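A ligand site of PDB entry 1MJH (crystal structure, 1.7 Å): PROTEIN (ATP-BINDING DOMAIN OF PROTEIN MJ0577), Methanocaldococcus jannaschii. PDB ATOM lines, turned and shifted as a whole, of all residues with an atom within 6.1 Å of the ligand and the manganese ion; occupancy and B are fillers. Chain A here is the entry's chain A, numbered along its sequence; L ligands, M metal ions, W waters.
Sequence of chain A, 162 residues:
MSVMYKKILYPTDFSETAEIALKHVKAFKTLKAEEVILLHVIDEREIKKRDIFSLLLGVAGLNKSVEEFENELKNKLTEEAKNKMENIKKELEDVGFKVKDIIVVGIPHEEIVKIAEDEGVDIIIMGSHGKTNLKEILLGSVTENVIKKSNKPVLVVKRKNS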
ATOM      1  N   TYR A  10      13.349  21.148 -13.328  1.00  0.00           N
ATOM      2  CA  TYR A  10      11.934  20.962 -12.997  1.00  0.00           C
ATOM      3  C   TYR A  10      11.259  22.320 -12.877  1.00  0.00           C
ATOM      4  O   TYR A  10      11.383  23.043 -11.878  1.00  0.00           O
ATOM      5  CB  TYR A  10      11.817  20.160 -11.670  1.00  0.00           C
ATOM      6  CG  TYR A  10      10.398  20.131 -11.128  1.00  0.00           C
ATOM      7  CD1 TYR A  10       9.324  19.774 -11.901  1.00  0.00           C
ATOM      8  CD2 TYR A  10      10.134  20.482  -9.813  1.00  0.00           C
ATOM      9  CE1 TYR A  10       8.021  19.735 -11.419  1.00  0.00           C
ATOM     10  CE2 TYR A  10       8.851  20.449  -9.300  1.00  0.00           C
ATOM     11  CZ  TYR A  10       7.799  20.103 -10.096  1.00  0.00           C
ATOM     12  OH  TYR A  10       6.520  20.090  -9.573  1.00  0.00           O
ATOM     13  N   PRO A  11      10.636  22.780 -13.951  1.00  0.00           N
ATOM     14  CA  PRO A  11       9.906  24.063 -13.937  1.00  0.00           C
ATOM     15  C   PRO A  11       8.492  23.860 -13.424  1.00  0.00           C
ATOM     16  O   PRO A  11       7.724  22.957 -13.835  1.00  0.00           O
ATOM     17  CB  PRO A  11       9.974  24.482 -15.413  1.00  0.00           C
ATOM     18  CG  PRO A  11       9.820  23.178 -16.138  1.00  0.00           C
ATOM     19  CD  PRO A  11      10.510  22.126 -15.291  1.00  0.00           C
ATOM     20  N   THR A  12       8.166  24.600 -12.344  1.00  0.00           N
ATOM     21  CA  THR A  12       6.837  24.480 -11.757  1.00  0.00           C
ATOM     22  C   THR A  12       6.039  25.774 -11.715  1.00  0.00           C
ATOM     23  O   THR A  12       6.613  26.829 -11.443  1.00  0.00           O
ATOM     24  CB  THR A  12       6.895  23.885 -10.315  1.00  0.00           C
ATOM     25  OG1 THR A  12       5.556  23.858  -9.813  1.00  0.00           O
ATOM     26  CG2 THR A  12       7.817  24.643  -9.388  1.00  0.00           C
ATOM     27  N   ASP A  13       4.751  25.673 -11.956  1.00  0.00           N
ATOM     28  CA  ASP A  13       3.802  26.769 -11.808  1.00  0.00           C
ATOM     29  C   ASP A  13       2.926  26.481 -10.574  1.00  0.00           C
ATOM     30  O   ASP A  13       1.883  27.112 -10.460  1.00  0.00           O
ATOM     31  CB  ASP A  13       2.842  26.874 -13.019  1.00  0.00           C
ATOM     32  CG  ASP A  13       2.221  25.516 -13.407  1.00  0.00           C
ATOM     33  OD1 ASP A  13       2.398  24.500 -12.698  1.00  0.00           O
ATOM     34  OD2 ASP A  13       1.532  25.568 -14.443  1.00  0.00           O
ATOM     35  N   SER A  15       0.956  24.073 -10.064  1.00  0.00           N
ATOM     36  CA  SER A  15      -0.349  23.526 -10.464  1.00  0.00           C
ATOM     37  C   SER A  15      -0.454  22.077 -10.035  1.00  0.00           C
ATOM     38  O   SER A  15       0.488  21.393  -9.657  1.00  0.00           O
ATOM     39  CB  SER A  15      -0.557  23.628 -11.973  1.00  0.00           C
ATOM     40  OG  SER A  15       0.370  22.801 -12.678  1.00  0.00           O
ATOM     41  N   THR A  17      -1.068  19.666 -12.038  1.00  0.00           N
ATOM     42  CA  THR A  17      -0.331  18.748 -12.956  1.00  0.00           C
ATOM     43  C   THR A  17       1.164  18.815 -12.731  1.00  0.00           C
ATOM     44  O   THR A  17       1.933  17.843 -12.674  1.00  0.00           O
ATOM     45  CB  THR A  17      -0.663  19.084 -14.437  1.00  0.00           C
ATOM     46  OG1 THR A  17      -2.075  19.011 -14.642  1.00  0.00           O
ATOM     47  CG2 THR A  17       0.049  18.070 -15.343  1.00  0.00           C
ATOM     48  N   ALA A  18       1.678  20.007 -12.372  1.00  0.00           N
ATOM     49  CA  ALA A  18       3.095  20.130 -12.001  1.00  0.00           C
ATOM     50  C   ALA A  18       3.426  19.274 -10.791  1.00  0.00           C
ATOM     51  O   ALA A  18       4.487  18.713 -10.600  1.00  0.00           O
ATOM     52  CB  ALA A  18       3.406  21.601 -11.695  1.00  0.00           C
ATOM     53  N   ALA A  21       4.044  15.931 -11.856  1.00  0.00           N
ATOM     54  CA  ALA A  21       5.415  15.848 -12.408  1.00  0.00           C
ATOM     55  C   ALA A  21       6.487  15.747 -11.357  1.00  0.00           C
ATOM     56  O   ALA A  21       7.530  15.118 -11.538  1.00  0.00           O
ATOM     57  CB  ALA A  21       5.696  17.018 -13.384  1.00  0.00           C
ATOM     58  N   LEU A  39      12.670  25.601 -10.848  1.00  0.00           N
ATOM     59  CA  LEU A  39      12.456  26.938 -11.411  1.00  0.00           C
ATOM     60  C   LEU A  39      11.003  27.352 -11.447  1.00  0.00           C
ATOM     61  O   LEU A  39      10.052  26.646 -11.853  1.00  0.00           O
ATOM     62  CB  LEU A  39      12.976  26.819 -12.885  1.00  0.00           C
ATOM     63  CG  LEU A  39      12.598  27.988 -13.783  1.00  0.00           C
ATOM     64  CD1 LEU A  39      13.259  29.303 -13.313  1.00  0.00           C
ATOM     65  CD2 LEU A  39      12.969  27.714 -15.249  1.00  0.00           C
ATOM     66  N   HIS A  40      10.716  28.589 -11.032  1.00  0.00           N
ATOM     67  CA  HIS A  40       9.441  29.212 -11.116  1.00  0.00           C
ATOM     68  C   HIS A  40       9.525  30.548 -11.863  1.00  0.00           C
ATOM     69  O   HIS A  40      10.476  31.304 -11.550  1.00  0.00           O
ATOM     70  CB  HIS A  40       8.730  29.479  -9.773  1.00  0.00           C
ATOM     71  CG  HIS A  40       7.386  30.102 -10.056  1.00  0.00           C
ATOM     72  ND1 HIS A  40       6.969  31.375  -9.746  1.00  0.00           N
ATOM     73  CD2 HIS A  40       6.319  29.541 -10.660  1.00  0.00           C
ATOM     74  CE1 HIS A  40       5.731  31.547 -10.154  1.00  0.00           C
ATOM     75  NE2 HIS A  40       5.314  30.427 -10.743  1.00  0.00           N
ATOM     76  N   VAL A  41       8.785  30.731 -12.932  1.00  0.00           N
ATOM     77  CA  VAL A  41       8.793  32.007 -13.649  1.00  0.00           C
ATOM     78  C   VAL A  41       7.534  32.786 -13.289  1.00  0.00           C
ATOM     79  O   VAL A  41       6.397  32.373 -13.503  1.00  0.00           O
ATOM     80  CB  VAL A  41       8.817  31.831 -15.193  1.00  0.00           C
ATOM     81  CG1 VAL A  41       8.866  33.207 -15.904  1.00  0.00           C
ATOM     82  CG2 VAL A  41       9.981  30.952 -15.577  1.00  0.00           C
ATOM     83  N   ILE A  42       7.726  34.049 -12.837  1.00  0.00           N
ATOM     84  CA  ILE A  42       6.570  34.932 -12.664  1.00  0.00           C
ATOM     85  C   ILE A  42       6.288  35.598 -14.013  1.00  0.00           C
ATOM     86  O   ILE A  42       7.115  36.297 -14.571  1.00  0.00           O
ATOM     87  CB  ILE A  42       6.843  36.032 -11.587  1.00  0.00           C
ATOM     88  CG1 ILE A  42       7.072  35.289 -10.276  1.00  0.00           C
ATOM     89  CG2 ILE A  42       5.657  37.004 -11.530  1.00  0.00           C
ATOM     90  CD1 ILE A  42       7.609  36.198  -9.134  1.00  0.00           C
ATOM     91  N   ASP A  43       5.096  35.306 -14.567  1.00  0.00           N
ATOM     92  CA  ASP A  43       4.864  35.725 -15.970  1.00  0.00           C
ATOM     93  C   ASP A  43       4.659  37.223 -16.067  1.00  0.00           C
ATOM     94  O   ASP A  43       3.703  37.780 -15.510  1.00  0.00           O
ATOM     95  CB  ASP A  43       3.661  34.948 -16.489  1.00  0.00           C
ATOM     96  CG  ASP A  43       3.361  35.222 -17.949  1.00  0.00           C
ATOM     97  OD1 ASP A  43       3.929  36.120 -18.611  1.00  0.00           O
ATOM     98  OD2 ASP A  43       2.514  34.453 -18.467  1.00  0.00           O
ATOM     99  N   PRO A 108       7.404  32.597 -19.328  1.00  0.00           N
ATOM    100  CA  PRO A 108       7.701  31.262 -18.836  1.00  0.00           C
ATOM    101  C   PRO A 108       8.403  30.359 -19.830  1.00  0.00           C
ATOM    102  O   PRO A 108       9.470  29.819 -19.518  1.00  0.00           O
ATOM    103  CB  PRO A 108       6.311  30.748 -18.453  1.00  0.00           C
ATOM    104  CG  PRO A 108       5.632  31.998 -17.932  1.00  0.00           C
ATOM    105  CD  PRO A 108       6.018  33.061 -18.953  1.00  0.00           C
ATOM    106  N   ILE A 112      12.344  29.027 -19.403  1.00  0.00           N
ATOM    107  CA  ILE A 112      12.611  27.584 -19.177  1.00  0.00           C
ATOM    108  C   ILE A 112      13.612  27.097 -20.217  1.00  0.00           C
ATOM    109  O   ILE A 112      14.574  26.435 -19.922  1.00  0.00           O
ATOM    110  CB  ILE A 112      11.281  26.785 -19.263  1.00  0.00           C
ATOM    111  CG1 ILE A 112      10.368  27.082 -18.075  1.00  0.00           C
ATOM    112  CG2 ILE A 112      11.634  25.278 -19.345  1.00  0.00           C
ATOM    113  CD1 ILE A 112       8.919  26.571 -18.309  1.00  0.00           C
ATOM    114  N   ILE A 125      11.702  17.944 -16.847  1.00  0.00           N
ATOM    115  CA  ILE A 125      10.544  17.122 -16.478  1.00  0.00           C
ATOM    116  C   ILE A 125       9.415  18.095 -16.116  1.00  0.00           C
ATOM    117  O   ILE A 125       9.586  18.970 -15.219  1.00  0.00           O
ATOM    118  CB  ILE A 125      10.886  16.233 -15.256  1.00  0.00           C
ATOM    119  CG1 ILE A 125      11.972  15.256 -15.646  1.00  0.00           C
ATOM    120  CG2 ILE A 125       9.619  15.449 -14.827  1.00  0.00           C
ATOM    121  CD1 ILE A 125      12.499  14.364 -14.486  1.00  0.00           C
ATOM    122  N   MET A 126       8.280  18.034 -16.784  1.00  0.00           N
ATOM    123  CA  MET A 126       7.250  19.069 -16.590  1.00  0.00           C
ATOM    124  C   MET A 126       5.843  18.534 -16.814  1.00  0.00           C
ATOM    125  O   MET A 126       5.699  17.500 -17.445  1.00  0.00           O
ATOM    126  CB  MET A 126       7.522  20.303 -17.520  1.00  0.00           C
ATOM    127  CG  MET A 126       7.368  20.037 -19.064  1.00  0.00           C
ATOM    128  SD  MET A 126       8.157  21.318 -20.192  1.00  0.00           S
ATOM    129  CE  MET A 126       7.243  22.765 -19.573  1.00  0.00           C
ATOM    130  N   GLY A 127       4.812  19.288 -16.425  1.00  0.00           N
ATOM    131  CA  GLY A 127       3.458  18.803 -16.723  1.00  0.00           C
ATOM    132  C   GLY A 127       3.026  19.018 -18.140  1.00  0.00           C
ATOM    133  O   GLY A 127       3.501  19.896 -18.860  1.00  0.00           O
ATOM    134  N   SER A 128       1.935  18.312 -18.530  1.00  0.00           N
ATOM    135  CA  SER A 128       1.358  18.629 -19.849  1.00  0.00           C
ATOM    136  C   SER A 128       0.520  19.892 -19.799  1.00  0.00           C
ATOM    137  O   SER A 128       0.238  20.520 -20.829  1.00  0.00           O
ATOM    138  CB  SER A 128       0.483  17.449 -20.331  1.00  0.00           C
ATOM    139  OG  SER A 128      -0.588  17.241 -19.390  1.00  0.00           O
ATOM    140  N   HIS A 129      -0.006  20.165 -18.609  1.00  0.00           N
ATOM    141  CA  HIS A 129      -0.935  21.276 -18.343  1.00  0.00           C
ATOM    142  C   HIS A 129      -0.551  21.941 -17.040  1.00  0.00           C
ATOM    143  O   HIS A 129       0.305  21.485 -16.293  1.00  0.00           O
ATOM    144  CB  HIS A 129      -2.384  20.748 -18.189  1.00  0.00           C
ATOM    145  CG  HIS A 129      -2.934  20.190 -19.486  1.00  0.00           C
ATOM    146  ND1 HIS A 129      -2.599  18.920 -19.956  1.00  0.00           N
ATOM    147  CD2 HIS A 129      -3.762  20.732 -20.391  1.00  0.00           C
ATOM    148  CE1 HIS A 129      -3.200  18.724 -21.113  1.00  0.00           C
ATOM    149  NE2 HIS A 129      -3.925  19.795 -21.402  1.00  0.00           N
ATOM    150  N   GLY A 130      -1.257  23.049 -16.727  1.00  0.00           N
ATOM    151  CA  GLY A 130      -0.804  23.919 -15.647  1.00  0.00           C
ATOM    152  C   GLY A 130      -1.967  24.557 -14.893  1.00  0.00           C
ATOM    153  O   GLY A 130      -2.984  23.894 -14.619  1.00  0.00           O
ATOM    154  N   LYS A 131      -1.815  25.860 -14.663  1.00  0.00           N
ATOM    155  CA  LYS A 131      -2.874  26.522 -13.885  1.00  0.00           C
ATOM    156  C   LYS A 131      -4.109  26.726 -14.715  1.00  0.00           C
ATOM    157  O   LYS A 131      -5.212  26.938 -14.147  1.00  0.00           O
ATOM    158  CB  LYS A 131      -2.297  27.855 -13.385  1.00  0.00           C
ATOM    159  CG  LYS A 131      -1.388  27.794 -12.181  1.00  0.00           C
ATOM    160  CD  LYS A 131      -2.121  27.225 -10.962  1.00  0.00           C
ATOM    161  CE  LYS A 131      -1.277  27.476  -9.707  1.00  0.00           C
ATOM    162  NZ  LYS A 131      -2.133  27.154  -8.507  1.00  0.00           N
ATOM    163  N   THR A 132      -4.053  26.770 -16.048  1.00  0.00           N
ATOM    164  CA  THR A 132      -5.280  27.001 -16.812  1.00  0.00           C
ATOM    165  C   THR A 132      -6.068  25.700 -16.894  1.00  0.00           C
ATOM    166  O   THR A 132      -7.266  25.592 -16.502  1.00  0.00           O
ATOM    167  CB  THR A 132      -5.032  27.476 -18.229  1.00  0.00           C
ATOM    168  OG1 THR A 132      -4.151  28.620 -18.104  1.00  0.00           O
ATOM    169  CG2 THR A 132      -6.294  27.901 -18.983  1.00  0.00           C
ATOM    170  N   ASN A 133      -5.398  24.687 -17.398  1.00  0.00           N
ATOM    171  CA  ASN A 133      -5.909  23.321 -17.483  1.00  0.00           C
ATOM    172  C   ASN A 133      -7.327  23.291 -18.015  1.00  0.00           C
ATOM    173  O   ASN A 133      -8.241  22.775 -17.337  1.00  0.00           O
ATOM    174  CB  ASN A 133      -5.662  22.452 -16.222  1.00  0.00           C
ATOM    175  CG  ASN A 133      -5.952  20.970 -16.523  1.00  0.00           C
ATOM    176  OD1 ASN A 133      -6.079  20.564 -17.665  1.00  0.00           O
ATOM    177  ND2 ASN A 133      -6.045  20.126 -15.474  1.00  0.00           N
ATOM    178  N   LEU A 134      -7.546  23.810 -19.213  1.00  0.00           N
ATOM    179  CA  LEU A 134      -8.879  23.782 -19.845  1.00  0.00           C
ATOM    180  C   LEU A 134      -9.084  22.406 -20.454  1.00  0.00           C
ATOM    181  O   LEU A 134      -8.176  21.870 -21.115  1.00  0.00           O
ATOM    182  CB  LEU A 134      -8.973  24.878 -20.878  1.00  0.00           C
ATOM    183  CG  LEU A 134     -10.281  25.002 -21.637  1.00  0.00           C
ATOM    184  CD1 LEU A 134     -11.383  25.447 -20.677  1.00  0.00           C
ATOM    185  CD2 LEU A 134     -10.100  26.060 -22.738  1.00  0.00           C
ATOM    186  N   ILE A 137      -8.231  21.815 -24.179  1.00  0.00           N
ATOM    187  CA  ILE A 137      -6.824  22.016 -24.578  1.00  0.00           C
ATOM    188  C   ILE A 137      -6.070  20.732 -24.279  1.00  0.00           C
ATOM    189  O   ILE A 137      -6.124  20.241 -23.160  1.00  0.00           O
ATOM    190  CB  ILE A 137      -6.240  23.211 -23.798  1.00  0.00           C
ATOM    191  CG1 ILE A 137      -6.896  24.523 -24.258  1.00  0.00           C
ATOM    192  CG2 ILE A 137      -4.717  23.267 -23.999  1.00  0.00           C
ATOM    193  CD1 ILE A 137      -6.540  24.965 -25.663  1.00  0.00           C
ATOM    194  N   LEU A 139      -2.728  20.179 -24.853  1.00  0.00           N
ATOM    195  CA  LEU A 139      -1.300  20.331 -24.402  1.00  0.00           C
ATOM    196  C   LEU A 139      -1.185  21.840 -24.113  1.00  0.00           C
ATOM    197  O   LEU A 139      -1.542  22.668 -24.992  1.00  0.00           O
ATOM    198  CB  LEU A 139      -0.370  19.997 -25.571  1.00  0.00           C
ATOM    199  CG  LEU A 139       1.118  20.099 -25.167  1.00  0.00           C
ATOM    200  CD1 LEU A 139       1.588  19.249 -23.997  1.00  0.00           C
ATOM    201  CD2 LEU A 139       1.929  19.758 -26.449  1.00  0.00           C
ATOM    202  N   GLY A 140      -0.709  22.136 -22.942  1.00  0.00           N
ATOM    203  CA  GLY A 140      -0.510  23.523 -22.542  1.00  0.00           C
ATOM    204  C   GLY A 140       0.500  24.235 -23.453  1.00  0.00           C
ATOM    205  O   GLY A 140       1.413  23.590 -23.966  1.00  0.00           O
ATOM    206  N   SER A 141       0.408  25.565 -23.502  1.00  0.00           N
ATOM    207  CA  SER A 141       1.293  26.301 -24.421  1.00  0.00           C
ATOM    208  C   SER A 141       2.719  26.417 -23.895  1.00  0.00           C
ATOM    209  O   SER A 141       3.620  26.504 -24.765  1.00  0.00           O
ATOM    210  CB  SER A 141       0.753  27.731 -24.695  1.00  0.00           C
ATOM    211  OG  SER A 141       0.812  28.583 -23.569  1.00  0.00           O
ATOM    212  N   VAL A 142       2.893  26.320 -22.580  1.00  0.00           N
ATOM    213  CA  VAL A 142       4.283  26.380 -22.078  1.00  0.00           C
ATOM    214  C   VAL A 142       5.034  25.114 -22.523  1.00  0.00           C
ATOM    215  O   VAL A 142       6.153  25.123 -23.031  1.00  0.00           O
ATOM    216  CB  VAL A 142       4.425  26.593 -20.586  1.00  0.00           C
ATOM    217  CG1 VAL A 142       5.896  26.663 -20.149  1.00  0.00           C
ATOM    218  CG2 VAL A 142       3.693  27.898 -20.198  1.00  0.00           C
ATOM    219  N   THR A 143       4.392  23.962 -22.285  1.00  0.00           N
ATOM    220  CA  THR A 143       5.033  22.683 -22.688  1.00  0.00           C
ATOM    221  C   THR A 143       5.186  22.555 -24.196  1.00  0.00           C
ATOM    222  O   THR A 143       6.302  22.192 -24.594  1.00  0.00           O
ATOM    223  CB  THR A 143       4.191  21.511 -22.157  1.00  0.00           C
ATOM    224  OG1 THR A 143       4.131  21.704 -20.727  1.00  0.00           O
ATOM    225  CG2 THR A 143       4.923  20.215 -22.428  1.00  0.00           C
ATOM    226  N   GLU A 144       4.205  22.989 -24.993  1.00  0.00           N
ATOM    227  CA  GLU A 144       4.377  22.954 -26.430  1.00  0.00           C
ATOM    228  C   GLU A 144       5.563  23.796 -26.861  1.00  0.00           C
ATOM    229  O   GLU A 144       6.386  23.336 -27.676  1.00  0.00           O
ATOM    230  CB  GLU A 144       3.087  23.356 -27.165  1.00  0.00           C
ATOM    231  CG  GLU A 144       3.240  23.114 -28.650  1.00  0.00           C
ATOM    232  CD  GLU A 144       1.941  23.167 -29.433  1.00  0.00           C
ATOM    233  OE1 GLU A 144       0.867  23.205 -28.789  1.00  0.00           O
ATOM    234  OE2 GLU A 144       2.061  23.176 -30.668  1.00  0.00           O
HETATM  235  P1  LIG L   1      -1.738  27.748 -20.809  1.00  0.00           P
HETATM  236  O1  LIG L   1      -1.296  27.764 -22.184  1.00  0.00           O
HETATM  237  O2  LIG L   1      -0.761  28.456 -19.980  1.00  0.00           O
HETATM  238  O3  LIG L   1      -3.034  28.427 -20.582  1.00  0.00           O
HETATM  239  P2  LIG L   1      -1.775  25.443 -18.957  1.00  0.00           P
HETATM  240  O4  LIG L   1      -2.864  24.460 -18.723  1.00  0.00           O
HETATM  241  O5  LIG L   1      -1.666  26.358 -17.826  1.00  0.00           O
HETATM  242  O6  LIG L   1      -1.992  26.213 -20.328  1.00  0.00           O
HETATM  243  P3  LIG L   1       1.168  25.047 -19.136  1.00  0.00           P
HETATM  244  O7  LIG L   1       1.688  24.855 -20.490  1.00  0.00           O
HETATM  245  O8  LIG L   1       1.335  26.419 -18.680  1.00  0.00           O
HETATM  246  O9  LIG L   1      -0.398  24.641 -19.153  1.00  0.00           O
HETATM  247  O10 LIG L   1       1.752  24.092 -18.057  1.00  0.00           O
HETATM  248  C1  LIG L   1       2.590  22.932 -18.455  1.00  0.00           C
HETATM  249  C2  LIG L   1       3.751  22.862 -17.475  1.00  0.00           C
HETATM  250  O11 LIG L   1       4.543  24.059 -17.763  1.00  0.00           O
HETATM  251  C3  LIG L   1       3.417  23.004 -15.981  1.00  0.00           C
HETATM  252  O12 LIG L   1       3.000  21.717 -15.422  1.00  0.00           O
HETATM  253  C4  LIG L   1       4.835  23.405 -15.463  1.00  0.00           C
HETATM  254  O13 LIG L   1       5.693  22.232 -15.375  1.00  0.00           O
HETATM  255  C5  LIG L   1       5.293  24.369 -16.612  1.00  0.00           C
HETATM  256  N1  LIG L   1       5.015  25.765 -16.323  1.00  0.00           N
HETATM  257  C6  LIG L   1       3.964  26.551 -16.669  1.00  0.00           C
HETATM  258  N2  LIG L   1       4.037  27.805 -16.263  1.00  0.00           N
HETATM  259  C7  LIG L   1       5.164  27.862 -15.591  1.00  0.00           C
HETATM  260  C8  LIG L   1       5.787  28.891 -14.903  1.00  0.00           C
HETATM  261  N3  LIG L   1       5.267  30.131 -14.844  1.00  0.00           N
HETATM  262  N4  LIG L   1       6.935  28.615 -14.304  1.00  0.00           N
HETATM  263  C9  LIG L   1       7.559  27.374 -14.341  1.00  0.00           C
HETATM  264  N5  LIG L   1       6.976  26.373 -14.971  1.00  0.00           N
HETATM  265  C10 LIG L   1       5.826  26.657 -15.564  1.00  0.00           C
HETATM  266 MN    MN M   1      -0.027  27.999 -17.814  1.00  0.00          MN
HETATM  267  O   HOH W   1      -3.138  27.023 -24.280  1.00  0.00           O
HETATM  268  O   HOH W   2       2.488  31.448 -15.206  1.00  0.00           O
HETATM  269  O   HOH W   3       1.803  29.497 -17.627  1.00  0.00           O
HETATM  270  O   HOH W   4      -5.042  26.898 -22.203  1.00  0.00           O
HETATM  271  O   HOH W   5      -5.001  24.511 -20.609  1.00  0.00           O
HETATM  272  O   HOH W   6       0.445  27.527 -15.527  1.00  0.00           O
HETATM  273  O   HOH W   7      -1.642  29.384 -16.959  1.00  0.00           O
HETATM  274  O   HOH W   8       0.404  30.752 -20.776  1.00  0.00           O
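The backbone carbonyl oxygen of Pro 11 sits at hydrogen-bond distance from an oxygen (O13) of the ligand, at 2.6 Å. O1 of the ligand is in hydrogen-bond range of N of Ser 141. The side-chain hydroxyl (OG) of Ser 141 sits at hydrogen-bond distance from an oxygen (O1) of the ligand (2.7 Å). An oxygen (O5) of the ligand lies close to the backbone NH of Thr 132 (3.0 Å). OG1 of Thr 132 sits at hydrogen-bond distance from O3 of the ligand, 2.7 Å away. N of Val 142 is in hydrogen-bond range of O7 of the ligand, 2.8 Å away. The backbone carbonyl oxygen (O) of His 129 lies within hydrogen-bond range of an oxygen (O12) of the ligand (2.8 Å). A nitrogen (N4) of the ligand is in hydrogen-bond range of the backbone NH (N) of Val 41, 3.1 Å away. The backbone carbonyl oxygen (O) of Val 41 lies within hydrogen-bond range of a nitrogen (N3) of the ligand (2.8 Å). The backbone NH of Asn 133 is in hydrogen-bond range of an oxygen (O4) of the ligand, at 2.9 Å. An oxygen (O4) of the ligand sits at hydrogen-bond distance from the backbone NH of Gly 130, 2.9 Å away. N of Thr 143 lies within hydrogen-bond range of O7 of the ligand (3.4 Å). N of Thr 12 lies within hydrogen-bond range of N5 of the ligand (3.4 Å). The backbone NH (N) of Gly 127 is in hydrogen-bond range of an oxygen (O12) of the ligand, at 3.2 Å. O5 of the ligand sits close to N of Lys 131 (3.2 Å).
The backbone carbonyl oxygen of Ile 137 lies within hydrogen-bond range of a ring nitrogen (NE2) of His 129 (2.9 Å). OG1 of Thr 143 sits at hydrogen-bond distance from O of Gly 127 (2.7 Å). The backbone NH (N) of Thr 12 lies within hydrogen-bond range of the backbone carbonyl oxygen (O) of Leu 39 (2.8 Å). N of Lys 131 is in hydrogen-bond range of OD2 of Asp 13 (3.4 Å). N of Gly 140 sits at hydrogen-bond distance from O of Ser 128, at 2.8 Å. OD1 of Asp 13 sits at hydrogen-bond distance from OG of Ser 15 (2.6 Å). The backbone NH (N) of Ala 18 lies within hydrogen-bond range of the side-chain hydroxyl (OG) of Ser 15 (3.1 Å). O of Ala 18 lies within hydrogen-bond range of OH of Tyr 10, 2.7 Å away.
Merely in contact with the ligand: Asp 13, Ser 15, Ala 18, Leu 39, His 40, Pro 108, Ile 112, Met 126, Ser 128 and Gly 140. Of the 32 residues printed, 22 come within 4 Å of the ligand. Along chain A the residues within 4 Å of the ligand span positions 11 to 143. The nearest printed residue that does not touch the ligand is Thr 17 (4.4 Å).
No residue comes within 4 Å of the manganese ion.
The manganese ion is bound by an oxygen (O8) of the ligand (2.3 Å), water W7 (2.3 Å), an oxygen (O5) of the ligand (2.3 Å), an oxygen (O2) of the ligand (2.3 Å), water W3 (2.4 Å) and water W6 (2.4 Å).
Water W6 lies within hydrogen-bond range of the side-chain carboxylate (OD2) of Asp 13 (2.5 Å) and the backbone NH (N) of Lys 131 (2.9 Å). Water W5 lies within hydrogen-bond range of O4 of the ligand (2.9 Å), N of Leu 134 (3.0 Å) and N of Asn 133 (3.2 Å).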
